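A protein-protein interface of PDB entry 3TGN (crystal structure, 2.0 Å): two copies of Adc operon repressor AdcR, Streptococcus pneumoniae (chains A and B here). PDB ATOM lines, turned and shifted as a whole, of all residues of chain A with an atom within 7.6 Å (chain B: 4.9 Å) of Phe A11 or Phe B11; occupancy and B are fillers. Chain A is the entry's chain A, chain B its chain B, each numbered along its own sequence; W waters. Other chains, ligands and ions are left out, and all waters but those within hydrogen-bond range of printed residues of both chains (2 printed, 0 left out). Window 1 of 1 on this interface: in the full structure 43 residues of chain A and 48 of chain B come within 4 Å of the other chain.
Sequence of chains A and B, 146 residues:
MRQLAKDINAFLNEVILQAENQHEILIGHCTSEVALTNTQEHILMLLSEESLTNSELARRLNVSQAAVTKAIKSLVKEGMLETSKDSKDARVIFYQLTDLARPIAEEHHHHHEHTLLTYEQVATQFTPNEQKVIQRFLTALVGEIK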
ATOM      1  N   LEU A   4      11.920  -4.564 -17.674  1.00  0.00           N
ATOM      2  CA  LEU A   4      12.926  -5.398 -17.034  1.00  0.00           C
ATOM      3  C   LEU A   4      14.221  -5.418 -17.845  1.00  0.00           C
ATOM      4  O   LEU A   4      15.306  -5.532 -17.282  1.00  0.00           O
ATOM      5  CB  LEU A   4      12.395  -6.816 -16.806  1.00  0.00           C
ATOM      6  CG  LEU A   4      13.390  -7.827 -16.233  1.00  0.00           C
ATOM      7  CD1 LEU A   4      13.974  -7.326 -14.917  1.00  0.00           C
ATOM      8  CD2 LEU A   4      12.728  -9.183 -16.056  1.00  0.00           C
ATOM      9  N   ALA A   5      14.106  -5.303 -19.164  1.00  0.00           N
ATOM     10  CA  ALA A   5      15.286  -5.238 -20.020  1.00  0.00           C
ATOM     11  C   ALA A   5      16.125  -4.013 -19.669  1.00  0.00           C
ATOM     12  O   ALA A   5      17.347  -4.093 -19.569  1.00  0.00           O
ATOM     13  CB  ALA A   5      14.893  -5.218 -21.489  1.00  0.00           C
ATOM     14  N   LYS A   6      15.460  -2.880 -19.472  1.00  0.00           N
ATOM     15  CA  LYS A   6      16.151  -1.652 -19.094  1.00  0.00           C
ATOM     16  C   LYS A   6      16.677  -1.737 -17.664  1.00  0.00           C
ATOM     17  O   LYS A   6      17.758  -1.234 -17.365  1.00  0.00           O
ATOM     18  CB  LYS A   6      15.227  -0.442 -19.255  1.00  0.00           C
ATOM     19  CG  LYS A   6      14.757  -0.214 -20.686  1.00  0.00           C
ATOM     20  CD  LYS A   6      13.802   0.967 -20.786  1.00  0.00           C
ATOM     21  CE  LYS A   6      13.264   1.113 -22.202  1.00  0.00           C
ATOM     22  NZ  LYS A   6      12.298   2.239 -22.323  1.00  0.00           N
ATOM     23  N   ASP A   7      15.910  -2.370 -16.779  1.00  0.00           N
ATOM     24  CA  ASP A   7      16.331  -2.523 -15.389  1.00  0.00           C
ATOM     25  C   ASP A   7      17.613  -3.342 -15.321  1.00  0.00           C
ATOM     26  O   ASP A   7      18.519  -3.041 -14.543  1.00  0.00           O
ATOM     27  CB  ASP A   7      15.244  -3.203 -14.554  1.00  0.00           C
ATOM     28  CG  ASP A   7      14.006  -2.340 -14.383  1.00  0.00           C
ATOM     29  OD1 ASP A   7      14.077  -1.124 -14.652  1.00  0.00           O
ATOM     30  OD2 ASP A   7      12.960  -2.883 -13.968  1.00  0.00           O
ATOM     31  N   ILE A   8      17.680  -4.385 -16.140  1.00  0.00           N
ATOM     32  CA  ILE A   8      18.870  -5.223 -16.216  1.00  0.00           C
ATOM     33  C   ILE A   8      20.091  -4.391 -16.583  1.00  0.00           C
ATOM     34  O   ILE A   8      21.119  -4.453 -15.913  1.00  0.00           O
ATOM     35  CB  ILE A   8      18.690  -6.364 -17.238  1.00  0.00           C
ATOM     36  CG1 ILE A   8      17.718  -7.413 -16.689  1.00  0.00           C
ATOM     37  CG2 ILE A   8      20.033  -7.003 -17.573  1.00  0.00           C
ATOM     38  CD1 ILE A   8      17.160  -8.346 -17.741  1.00  0.00           C
ATOM     39  N   ASN A   9      19.972  -3.609 -17.650  1.00  0.00           N
ATOM     40  CA  ASN A   9      21.070  -2.758 -18.086  1.00  0.00           C
ATOM     41  C   ASN A   9      21.503  -1.783 -16.996  1.00  0.00           C
ATOM     42  O   ASN A   9      22.695  -1.577 -16.768  1.00  0.00           O
ATOM     43  CB  ASN A   9      20.685  -1.996 -19.354  1.00  0.00           C
ATOM     44  CG  ASN A   9      21.871  -1.325 -20.009  1.00  0.00           C
ATOM     45  OD1 ASN A   9      22.699  -1.984 -20.636  1.00  0.00           O
ATOM     46  ND2 ASN A   9      21.958  -0.007 -19.869  1.00  0.00           N
ATOM     47  N   ALA A  10      20.526  -1.184 -16.320  1.00  0.00           N
ATOM     48  CA  ALA A  10      20.819  -0.231 -15.258  1.00  0.00           C
ATOM     49  C   ALA A  10      21.528  -0.941 -14.117  1.00  0.00           C
ATOM     50  O   ALA A  10      22.487  -0.420 -13.546  1.00  0.00           O
ATOM     51  CB  ALA A  10      19.543   0.435 -14.766  1.00  0.00           C
ATOM     52  N   PHE A  11      21.059  -2.141 -13.800  1.00  0.00           N
ATOM     53  CA  PHE A  11      21.642  -2.920 -12.721  1.00  0.00           C
ATOM     54  C   PHE A  11      23.103  -3.268 -13.001  1.00  0.00           C
ATOM     55  O   PHE A  11      23.965  -3.096 -12.142  1.00  0.00           O
ATOM     56  CB  PHE A  11      20.837  -4.196 -12.486  1.00  0.00           C
ATOM     57  CG  PHE A  11      21.389  -5.054 -11.393  1.00  0.00           C
ATOM     58  CD1 PHE A  11      21.140  -4.746 -10.068  1.00  0.00           C
ATOM     59  CD2 PHE A  11      22.170  -6.157 -11.688  1.00  0.00           C
ATOM     60  CE1 PHE A  11      21.651  -5.527  -9.056  1.00  0.00           C
ATOM     61  CE2 PHE A  11      22.687  -6.943 -10.680  1.00  0.00           C
ATOM     62  CZ  PHE A  11      22.426  -6.629  -9.361  1.00  0.00           C
ATOM     63  N   LEU A  12      23.375  -3.755 -14.206  1.00  0.00           N
ATOM     64  CA  LEU A  12      24.733  -4.143 -14.573  1.00  0.00           C
ATOM     65  C   LEU A  12      25.695  -2.958 -14.487  1.00  0.00           C
ATOM     66  O   LEU A  12      26.836  -3.110 -14.048  1.00  0.00           O
ATOM     67  CB  LEU A  12      24.768  -4.779 -15.967  1.00  0.00           C
ATOM     68  CG  LEU A  12      24.100  -6.152 -16.102  1.00  0.00           C
ATOM     69  CD1 LEU A  12      24.082  -6.615 -17.555  1.00  0.00           C
ATOM     70  CD2 LEU A  12      24.770  -7.194 -15.212  1.00  0.00           C
ATOM     71  N   ASN A  13      25.226  -1.782 -14.900  1.00  0.00           N
ATOM     72  CA  ASN A  13      26.025  -0.567 -14.801  1.00  0.00           C
ATOM     73  C   ASN A  13      26.353  -0.222 -13.349  1.00  0.00           C
ATOM     74  O   ASN A  13      27.458   0.222 -13.046  1.00  0.00           O
ATOM     75  CB  ASN A  13      25.322   0.615 -15.478  1.00  0.00           C
ATOM     76  CG  ASN A  13      25.267   0.477 -16.990  1.00  0.00           C
ATOM     77  OD1 ASN A  13      26.076  -0.229 -17.594  1.00  0.00           O
ATOM     78  ND2 ASN A  13      24.314   1.164 -17.611  1.00  0.00           N
ATOM     79  N   GLU A  14      25.391  -0.434 -12.457  1.00  0.00           N
ATOM     80  CA  GLU A  14      25.583  -0.144 -11.043  1.00  0.00           C
ATOM     81  C   GLU A  14      26.611  -1.088 -10.427  1.00  0.00           C
ATOM     82  O   GLU A  14      27.458  -0.669  -9.639  1.00  0.00           O
ATOM     83  CB  GLU A  14      24.260  -0.238 -10.284  1.00  0.00           C
ATOM     84  CG  GLU A  14      24.358   0.237  -8.849  1.00  0.00           C
ATOM     85  CD  GLU A  14      24.709   1.708  -8.755  1.00  0.00           C
ATOM     86  OE1 GLU A  14      24.162   2.501  -9.550  1.00  0.00           O
ATOM     87  OE2 GLU A  14      25.530   2.072  -7.890  1.00  0.00           O
ATOM     88  N   VAL A  15      26.537  -2.363 -10.795  1.00  0.00           N
ATOM     89  CA  VAL A  15      27.516  -3.339 -10.335  1.00  0.00           C
ATOM     90  C   VAL A  15      28.917  -2.942 -10.782  1.00  0.00           C
ATOM     91  O   VAL A  15      29.864  -2.952  -9.995  1.00  0.00           O
ATOM     92  CB  VAL A  15      27.201  -4.746 -10.866  1.00  0.00           C
ATOM     93  CG1 VAL A  15      28.348  -5.688 -10.564  1.00  0.00           C
ATOM     94  CG2 VAL A  15      25.917  -5.269 -10.252  1.00  0.00           C
ATOM     95  N   ILE A  16      29.041  -2.592 -12.056  1.00  0.00           N
ATOM     96  CA  ILE A  16      30.316  -2.166 -12.609  1.00  0.00           C
ATOM     97  C   ILE A  16      30.826  -0.910 -11.901  1.00  0.00           C
ATOM     98  O   ILE A  16      32.006  -0.812 -11.558  1.00  0.00           O
ATOM     99  CB  ILE A  16      30.201  -1.931 -14.123  1.00  0.00           C
ATOM    100  CG1 ILE A  16      29.890  -3.253 -14.831  1.00  0.00           C
ATOM    101  CG2 ILE A  16      31.475  -1.300 -14.670  1.00  0.00           C
ATOM    102  CD1 ILE A  16      29.669  -3.119 -16.333  1.00  0.00           C
ATOM    103  N   LEU A  17      29.932   0.043 -11.667  1.00  0.00           N
ATOM    104  CA  LEU A  17      30.288   1.239 -10.915  1.00  0.00           C
ATOM    105  C   LEU A  17      30.789   0.888  -9.513  1.00  0.00           C
ATOM    106  O   LEU A  17      31.811   1.405  -9.064  1.00  0.00           O
ATOM    107  CB  LEU A  17      29.088   2.181 -10.822  1.00  0.00           C
ATOM    108  CG  LEU A  17      29.271   3.451  -9.993  1.00  0.00           C
ATOM    109  CD1 LEU A  17      30.423   4.274 -10.532  1.00  0.00           C
ATOM    110  CD2 LEU A  17      27.987   4.270  -9.977  1.00  0.00           C
ATOM    111  N   GLN A  18      30.068   0.006  -8.827  1.00  0.00           N
ATOM    112  CA  GLN A  18      30.409  -0.365  -7.455  1.00  0.00           C
ATOM    113  C   GLN A  18      31.704  -1.173  -7.358  1.00  0.00           C
ATOM    114  O   GLN A  18      32.382  -1.151  -6.328  1.00  0.00           O
ATOM    115  CB  GLN A  18      29.257  -1.142  -6.807  1.00  0.00           C
ATOM    116  CG  GLN A  18      27.991  -0.321  -6.603  1.00  0.00           C
ATOM    117  CD  GLN A  18      28.174   0.789  -5.587  1.00  0.00           C
ATOM    118  OE1 GLN A  18      29.094   0.750  -4.771  1.00  0.00           O
ATOM    119  NE2 GLN A  18      27.298   1.787  -5.632  1.00  0.00           N
ATOM    120  N   ILE A  25      32.395  -7.714  -5.685  1.00  0.00           N
ATOM    121  CA  ILE A  25      31.638  -6.782  -4.869  1.00  0.00           C
ATOM    122  C   ILE A  25      31.527  -7.320  -3.452  1.00  0.00           C
ATOM    123  O   ILE A  25      31.251  -8.500  -3.252  1.00  0.00           O
ATOM    124  CB  ILE A  25      30.223  -6.559  -5.425  1.00  0.00           C
ATOM    125  CG1 ILE A  25      30.255  -5.528  -6.556  1.00  0.00           C
ATOM    126  CG2 ILE A  25      29.285  -6.099  -4.314  1.00  0.00           C
ATOM    127  CD1 ILE A  25      28.894  -5.189  -7.102  1.00  0.00           C
ATOM    128  N   PHE A 137      16.733 -17.005 -13.820  1.00  0.00           N
ATOM    129  CA  PHE A 137      16.996 -15.704 -14.412  1.00  0.00           C
ATOM    130  C   PHE A 137      18.490 -15.403 -14.457  1.00  0.00           C
ATOM    131  O   PHE A 137      19.029 -15.059 -15.511  1.00  0.00           O
ATOM    132  CB  PHE A 137      16.252 -14.604 -13.654  1.00  0.00           C
ATOM    133  CG  PHE A 137      16.755 -13.223 -13.951  1.00  0.00           C
ATOM    134  CD1 PHE A 137      16.444 -12.600 -15.148  1.00  0.00           C
ATOM    135  CD2 PHE A 137      17.546 -12.548 -13.034  1.00  0.00           C
ATOM    136  CE1 PHE A 137      16.906 -11.326 -15.423  1.00  0.00           C
ATOM    137  CE2 PHE A 137      18.014 -11.275 -13.305  1.00  0.00           C
ATOM    138  CZ  PHE A 137      17.694 -10.664 -14.501  1.00  0.00           C
ATOM    139  N   LEU A 138      19.155 -15.539 -13.311  1.00  0.00           N
ATOM    140  CA  LEU A 138      20.589 -15.285 -13.228  1.00  0.00           C
ATOM    141  C   LEU A 138      21.352 -16.128 -14.242  1.00  0.00           C
ATOM    142  O   LEU A 138      22.269 -15.642 -14.908  1.00  0.00           O
ATOM    143  CB  LEU A 138      21.109 -15.567 -11.815  1.00  0.00           C
ATOM    144  CG  LEU A 138      20.592 -14.658 -10.697  1.00  0.00           C
ATOM    145  CD1 LEU A 138      21.208 -15.051  -9.357  1.00  0.00           C
ATOM    146  CD2 LEU A 138      20.879 -13.200 -11.016  1.00  0.00           C
ATOM    147  N   THR A 139      20.965 -17.393 -14.357  1.00  0.00           N
ATOM    148  CA  THR A 139      21.629 -18.317 -15.269  1.00  0.00           C
ATOM    149  C   THR A 139      21.377 -17.942 -16.732  1.00  0.00           C
ATOM    150  O   THR A 139      22.289 -17.996 -17.560  1.00  0.00           O
ATOM    151  CB  THR A 139      21.200 -19.779 -14.998  1.00  0.00           C
ATOM    152  OG1 THR A 139      21.544 -20.134 -13.651  1.00  0.00           O
ATOM    153  CG2 THR A 139      21.893 -20.731 -15.954  1.00  0.00           C
ATOM    154  N   LEU A 141      20.601 -14.939 -17.900  1.00  0.00           N
ATOM    155  CA  LEU A 141      21.262 -13.666 -18.169  1.00  0.00           C
ATOM    156  C   LEU A 141      22.749 -13.854 -18.447  1.00  0.00           C
ATOM    157  O   LEU A 141      23.270 -13.366 -19.452  1.00  0.00           O
ATOM    158  CB  LEU A 141      21.068 -12.704 -16.994  1.00  0.00           C
ATOM    159  CG  LEU A 141      21.724 -11.330 -17.133  1.00  0.00           C
ATOM    160  CD1 LEU A 141      21.310 -10.678 -18.445  1.00  0.00           C
ATOM    161  CD2 LEU A 141      21.360 -10.445 -15.949  1.00  0.00           C
ATOM    162  N   VAL A 142      23.433 -14.554 -17.551  1.00  0.00           N
ATOM    163  CA  VAL A 142      24.855 -14.808 -17.726  1.00  0.00           C
ATOM    164  C   VAL A 142      25.099 -15.568 -19.025  1.00  0.00           C
ATOM    165  O   VAL A 142      26.061 -15.295 -19.744  1.00  0.00           O
ATOM    166  CB  VAL A 142      25.442 -15.589 -16.537  1.00  0.00           C
ATOM    167  CG1 VAL A 142      26.757 -16.240 -16.919  1.00  0.00           C
ATOM    168  CG2 VAL A 142      25.624 -14.666 -15.340  1.00  0.00           C
ATOM    169  N   ILE A 145      25.487 -13.228 -21.814  1.00  0.00           N
ATOM    170  CA  ILE A 145      26.582 -12.266 -21.728  1.00  0.00           C
ATOM    171  C   ILE A 145      27.913 -12.850 -22.200  1.00  0.00           C
ATOM    172  O   ILE A 145      28.480 -13.738 -21.560  1.00  0.00           O
ATOM    173  CB  ILE A 145      26.738 -11.718 -20.306  1.00  0.00           C
ATOM    174  CG1 ILE A 145      25.502 -10.902 -19.919  1.00  0.00           C
ATOM    175  CG2 ILE A 145      27.988 -10.869 -20.205  1.00  0.00           C
ATOM    176  CD1 ILE A 145      25.510 -10.427 -18.480  1.00  0.00           C
ATOM    177  N   ASP B   7      24.602 -18.270  -5.409  1.00  0.00           N
ATOM    178  CA  ASP B   7      24.442 -17.964  -6.828  1.00  0.00           C
ATOM    179  C   ASP B   7      24.620 -16.476  -7.103  1.00  0.00           C
ATOM    180  O   ASP B   7      25.156 -16.090  -8.140  1.00  0.00           O
ATOM    181  CB  ASP B   7      23.072 -18.414  -7.332  1.00  0.00           C
ATOM    182  CG  ASP B   7      22.879 -19.908  -7.227  1.00  0.00           C
ATOM    183  OD1 ASP B   7      23.889 -20.641  -7.211  1.00  0.00           O
ATOM    184  OD2 ASP B   7      21.715 -20.351  -7.165  1.00  0.00           O
ATOM    185  N   ILE B   8      24.152 -15.646  -6.178  1.00  0.00           N
ATOM    186  CA  ILE B   8      24.246 -14.196  -6.323  1.00  0.00           C
ATOM    187  C   ILE B   8      25.701 -13.742  -6.324  1.00  0.00           C
ATOM    188  O   ILE B   8      26.099 -12.876  -7.107  1.00  0.00           O
ATOM    189  CB  ILE B   8      23.504 -13.477  -5.178  1.00  0.00           C
ATOM    190  CG1 ILE B   8      21.993 -13.691  -5.298  1.00  0.00           C
ATOM    191  CG2 ILE B   8      23.834 -11.989  -5.169  1.00  0.00           C
ATOM    192  CD1 ILE B   8      21.214 -13.160  -4.106  1.00  0.00           C
ATOM    193  N   ASN B   9      26.488 -14.325  -5.430  1.00  0.00           N
ATOM    194  CA  ASN B   9      27.902 -14.004  -5.343  1.00  0.00           C
ATOM    195  C   ASN B   9      28.634 -14.391  -6.623  1.00  0.00           C
ATOM    196  O   ASN B   9      29.423 -13.611  -7.164  1.00  0.00           O
ATOM    197  CB  ASN B   9      28.529 -14.715  -4.148  1.00  0.00           C
ATOM    198  CG  ASN B   9      29.932 -14.235  -3.861  1.00  0.00           C
ATOM    199  OD1 ASN B   9      30.128 -13.175  -3.269  1.00  0.00           O
ATOM    200  ND2 ASN B   9      30.920 -15.014  -4.280  1.00  0.00           N
ATOM    201  N   ALA B  10      28.369 -15.600  -7.105  1.00  0.00           N
ATOM    202  CA  ALA B  10      29.017 -16.084  -8.315  1.00  0.00           C
ATOM    203  C   ALA B  10      28.579 -15.255  -9.520  1.00  0.00           C
ATOM    204  O   ALA B  10      29.377 -14.967 -10.410  1.00  0.00           O
ATOM    205  CB  ALA B  10      28.718 -17.562  -8.529  1.00  0.00           C
ATOM    206  N   PHE B  11      27.309 -14.865  -9.532  1.00  0.00           N
ATOM    207  CA  PHE B  11      26.760 -14.040 -10.601  1.00  0.00           C
ATOM    208  C   PHE B  11      27.462 -12.689 -10.679  1.00  0.00           C
ATOM    209  O   PHE B  11      27.876 -12.258 -11.757  1.00  0.00           O
ATOM    210  CB  PHE B  11      25.252 -13.850 -10.401  1.00  0.00           C
ATOM    211  CG  PHE B  11      24.669 -12.709 -11.189  1.00  0.00           C
ATOM    212  CD1 PHE B  11      24.406 -12.841 -12.542  1.00  0.00           C
ATOM    213  CD2 PHE B  11      24.363 -11.508 -10.567  1.00  0.00           C
ATOM    214  CE1 PHE B  11      23.859 -11.793 -13.264  1.00  0.00           C
ATOM    215  CE2 PHE B  11      23.818 -10.454 -11.285  1.00  0.00           C
ATOM    216  CZ  PHE B  11      23.568 -10.598 -12.636  1.00  0.00           C
ATOM    217  N   LEU B  12      27.592 -12.026  -9.534  1.00  0.00           N
ATOM    218  CA  LEU B  12      28.262 -10.731  -9.482  1.00  0.00           C
ATOM    219  C   LEU B  12      29.717 -10.849  -9.928  1.00  0.00           C
ATOM    220  O   LEU B  12      30.204 -10.011 -10.686  1.00  0.00           O
ATOM    221  CB  LEU B  12      28.161 -10.116  -8.085  1.00  0.00           C
ATOM    222  CG  LEU B  12      26.732  -9.782  -7.642  1.00  0.00           C
ATOM    223  CD1 LEU B  12      26.702  -9.307  -6.197  1.00  0.00           C
ATOM    224  CD2 LEU B  12      26.089  -8.747  -8.570  1.00  0.00           C
ATOM    225  N   ASN B  13      30.405 -11.889  -9.461  1.00  0.00           N
ATOM    226  CA  ASN B  13      31.757 -12.183  -9.935  1.00  0.00           C
ATOM    227  C   ASN B  13      31.820 -12.255 -11.457  1.00  0.00           C
ATOM    228  O   ASN B  13      32.710 -11.674 -12.077  1.00  0.00           O
ATOM    229  CB  ASN B  13      32.271 -13.501  -9.351  1.00  0.00           C
ATOM    230  CG  ASN B  13      32.723 -13.367  -7.914  1.00  0.00           C
ATOM    231  OD1 ASN B  13      32.600 -12.306  -7.311  1.00  0.00           O
ATOM    232  ND2 ASN B  13      33.246 -14.454  -7.354  1.00  0.00           N
ATOM    233  N   GLU B  14      30.873 -12.973 -12.052  1.00  0.00           N
ATOM    234  CA  GLU B  14      30.846 -13.164 -13.498  1.00  0.00           C
ATOM    235  C   GLU B  14      30.594 -11.851 -14.241  1.00  0.00           C
ATOM    236  O   GLU B  14      31.241 -11.569 -15.246  1.00  0.00           O
ATOM    237  CB  GLU B  14      29.795 -14.209 -13.888  1.00  0.00           C
ATOM    238  CG  GLU B  14      29.923 -14.712 -15.318  1.00  0.00           C
ATOM    239  CD  GLU B  14      31.221 -15.459 -15.559  1.00  0.00           C
ATOM    240  OE1 GLU B  14      31.596 -16.291 -14.707  1.00  0.00           O
ATOM    241  OE2 GLU B  14      31.872 -15.212 -16.596  1.00  0.00           O
ATOM    242  N   VAL B  15      29.649 -11.054 -13.748  1.00  0.00           N
ATOM    243  CA  VAL B  15      29.380  -9.752 -14.343  1.00  0.00           C
ATOM    244  C   VAL B  15      30.667  -8.944 -14.443  1.00  0.00           C
ATOM    245  O   VAL B  15      31.035  -8.469 -15.515  1.00  0.00           O
ATOM    246  CB  VAL B  15      28.339  -8.948 -13.526  1.00  0.00           C
ATOM    247  CG1 VAL B  15      28.330  -7.488 -13.957  1.00  0.00           C
ATOM    248  CG2 VAL B  15      26.961  -9.557 -13.681  1.00  0.00           C
ATOM    249  N   LEU B 138      16.012  -7.476  -8.120  1.00  0.00           N
ATOM    250  CA  LEU B 138      17.069  -6.548  -8.515  1.00  0.00           C
ATOM    251  C   LEU B 138      17.049  -5.284  -7.656  1.00  0.00           C
ATOM    252  O   LEU B 138      18.096  -4.738  -7.306  1.00  0.00           O
ATOM    253  CB  LEU B 138      16.952  -6.193  -9.998  1.00  0.00           C
ATOM    254  CG  LEU B 138      17.135  -7.347 -10.986  1.00  0.00           C
ATOM    255  CD1 LEU B 138      16.885  -6.887 -12.417  1.00  0.00           C
ATOM    256  CD2 LEU B 138      18.527  -7.948 -10.846  1.00  0.00           C
ATOM    257  N   LEU B 141      18.430  -6.276  -4.191  1.00  0.00           N
ATOM    258  CA  LEU B 141      19.860  -6.547  -4.299  1.00  0.00           C
ATOM    259  C   LEU B 141      20.663  -5.258  -4.464  1.00  0.00           C
ATOM    260  O   LEU B 141      21.643  -5.033  -3.756  1.00  0.00           O
ATOM    261  CB  LEU B 141      20.138  -7.501  -5.464  1.00  0.00           C
ATOM    262  CG  LEU B 141      21.589  -7.946  -5.643  1.00  0.00           C
ATOM    263  CD1 LEU B 141      22.158  -8.433  -4.320  1.00  0.00           C
ATOM    264  CD2 LEU B 141      21.693  -9.036  -6.709  1.00  0.00           C
ATOM    265  N   VAL B 142      20.242  -4.409  -5.395  1.00  0.00           N
ATOM    266  CA  VAL B 142      20.955  -3.161  -5.649  1.00  0.00           C
ATOM    267  C   VAL B 142      20.929  -2.252  -4.421  1.00  0.00           C
ATOM    268  O   VAL B 142      21.823  -1.427  -4.228  1.00  0.00           O
ATOM    269  CB  VAL B 142      20.377  -2.410  -6.864  1.00  0.00           C
ATOM    270  CG1 VAL B 142      19.055  -1.749  -6.505  1.00  0.00           C
ATOM    271  CG2 VAL B 142      21.370  -1.376  -7.369  1.00  0.00           C
ATOM    272  N   ILE B 145      23.837  -3.348  -2.258  1.00  0.00           N
ATOM    273  CA  ILE B 145      25.113  -3.094  -2.913  1.00  0.00           C
ATOM    274  C   ILE B 145      25.546  -1.631  -2.820  1.00  0.00           C
ATOM    275  O   ILE B 145      26.731  -1.340  -2.648  1.00  0.00           O
ATOM    276  CB  ILE B 145      25.065  -3.527  -4.390  1.00  0.00           C
ATOM    277  CG1 ILE B 145      24.945  -5.049  -4.486  1.00  0.00           C
ATOM    278  CG2 ILE B 145      26.295  -3.046  -5.132  1.00  0.00           C
ATOM    279  CD1 ILE B 145      24.803  -5.567  -5.904  1.00  0.00           C
HETATM  280  O   HOH W   1      31.295 -10.070  -6.653  1.00  0.00           O
HETATM  281  O   HOH W   2      29.694 -10.443  -3.949  1.00  0.00           O
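Of the 13 printed residues of chain B, 8 touch a printed residue of chain A.
Printed residues of chain B that touch a printed residue of chain A: Phe B11, Leu B12, Glu B14, Val B15, Leu B138, Leu B141, Val B142 and Ile B145.
Along chain B the printed residues that touch a printed residue of chain A span positions 11 to 145.
Hydrophobic or aromatic side chains of chain A within 4 Å of the printed part of chain B: Leu A4, Phe A11, Leu A12, Val A15, Ile A25, Leu A138, Leu A141 and Val A142.
Among the printed residues, 13 pairs touch across the chains.
Among the printed residues, no Asp or Glu carboxylate lies within 4 Å of a Lys or Arg side-chain nitrogen of the other chain.
Water W2 lies within hydrogen-bond range of the backbone carbonyl oxygen (O) of Ile A25 (2.6 Å) and the side-chain amide oxygen (OD1) of Asn B9 (2.8 Å).
Water W1 bridges OD1 of Asn B13 (2.7 Å) and N of Ile A25 (2.8 Å).
Among the printed residues, pairs that only touch across the chains: Gln A18 with Ile B145, Val A142 with Phe B11, Leu A12 with Val B15, Phe A11 with Leu B141, Glu A14 with Val B142, Phe A11 with Phe B11, Leu A138 with Phe B11, Val A15 with Val B15, Leu A4 with Leu B138, Val A142 with Glu B14, Val A15 with Leu B12, Ile A25 with Ile B145 and Leu A141 with Phe B11.
Of the printed residues of chain B, Phe A11 touches Phe B11 (3.7 Å) and Leu B141 (3.7 Å).
Printed residues of chain B within 4 Å of Ile A25: Ile B145 (3.9 Å).
No residue of chain A comes within 4 Å of Ala B10.
Printed residues of chain A within 4 Å of Glu B14: Val A142.
Printed residues of chain A within 4 Å of Val B15: Leu A12 (3.6 Å) and Val A15 (3.8 Å).
The nearest printed residue of chain B that does not touch Gln A18 is Val B142 (6.5 Å).
The side-chain carboxylate of Glu A14 is in hydrogen-bond range of the side-chain amide nitrogen of Gln A18, at 2.9 Å.
Phe B11 touches its own counterpart, Phe A11.
Leu A12 touches Val B15, and with the chains exchanged Val A15 touches Leu B12.
Glu A14 touches Val B142, and with the chains exchanged Val A142 touches Glu B14.
Val A15 touches its own counterpart, Val B15.
13 positions are printed for both chains.
Of the 13 pairs that touch across the chains among the printed residues, 8 have their exchanged pair printed and touching as well.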
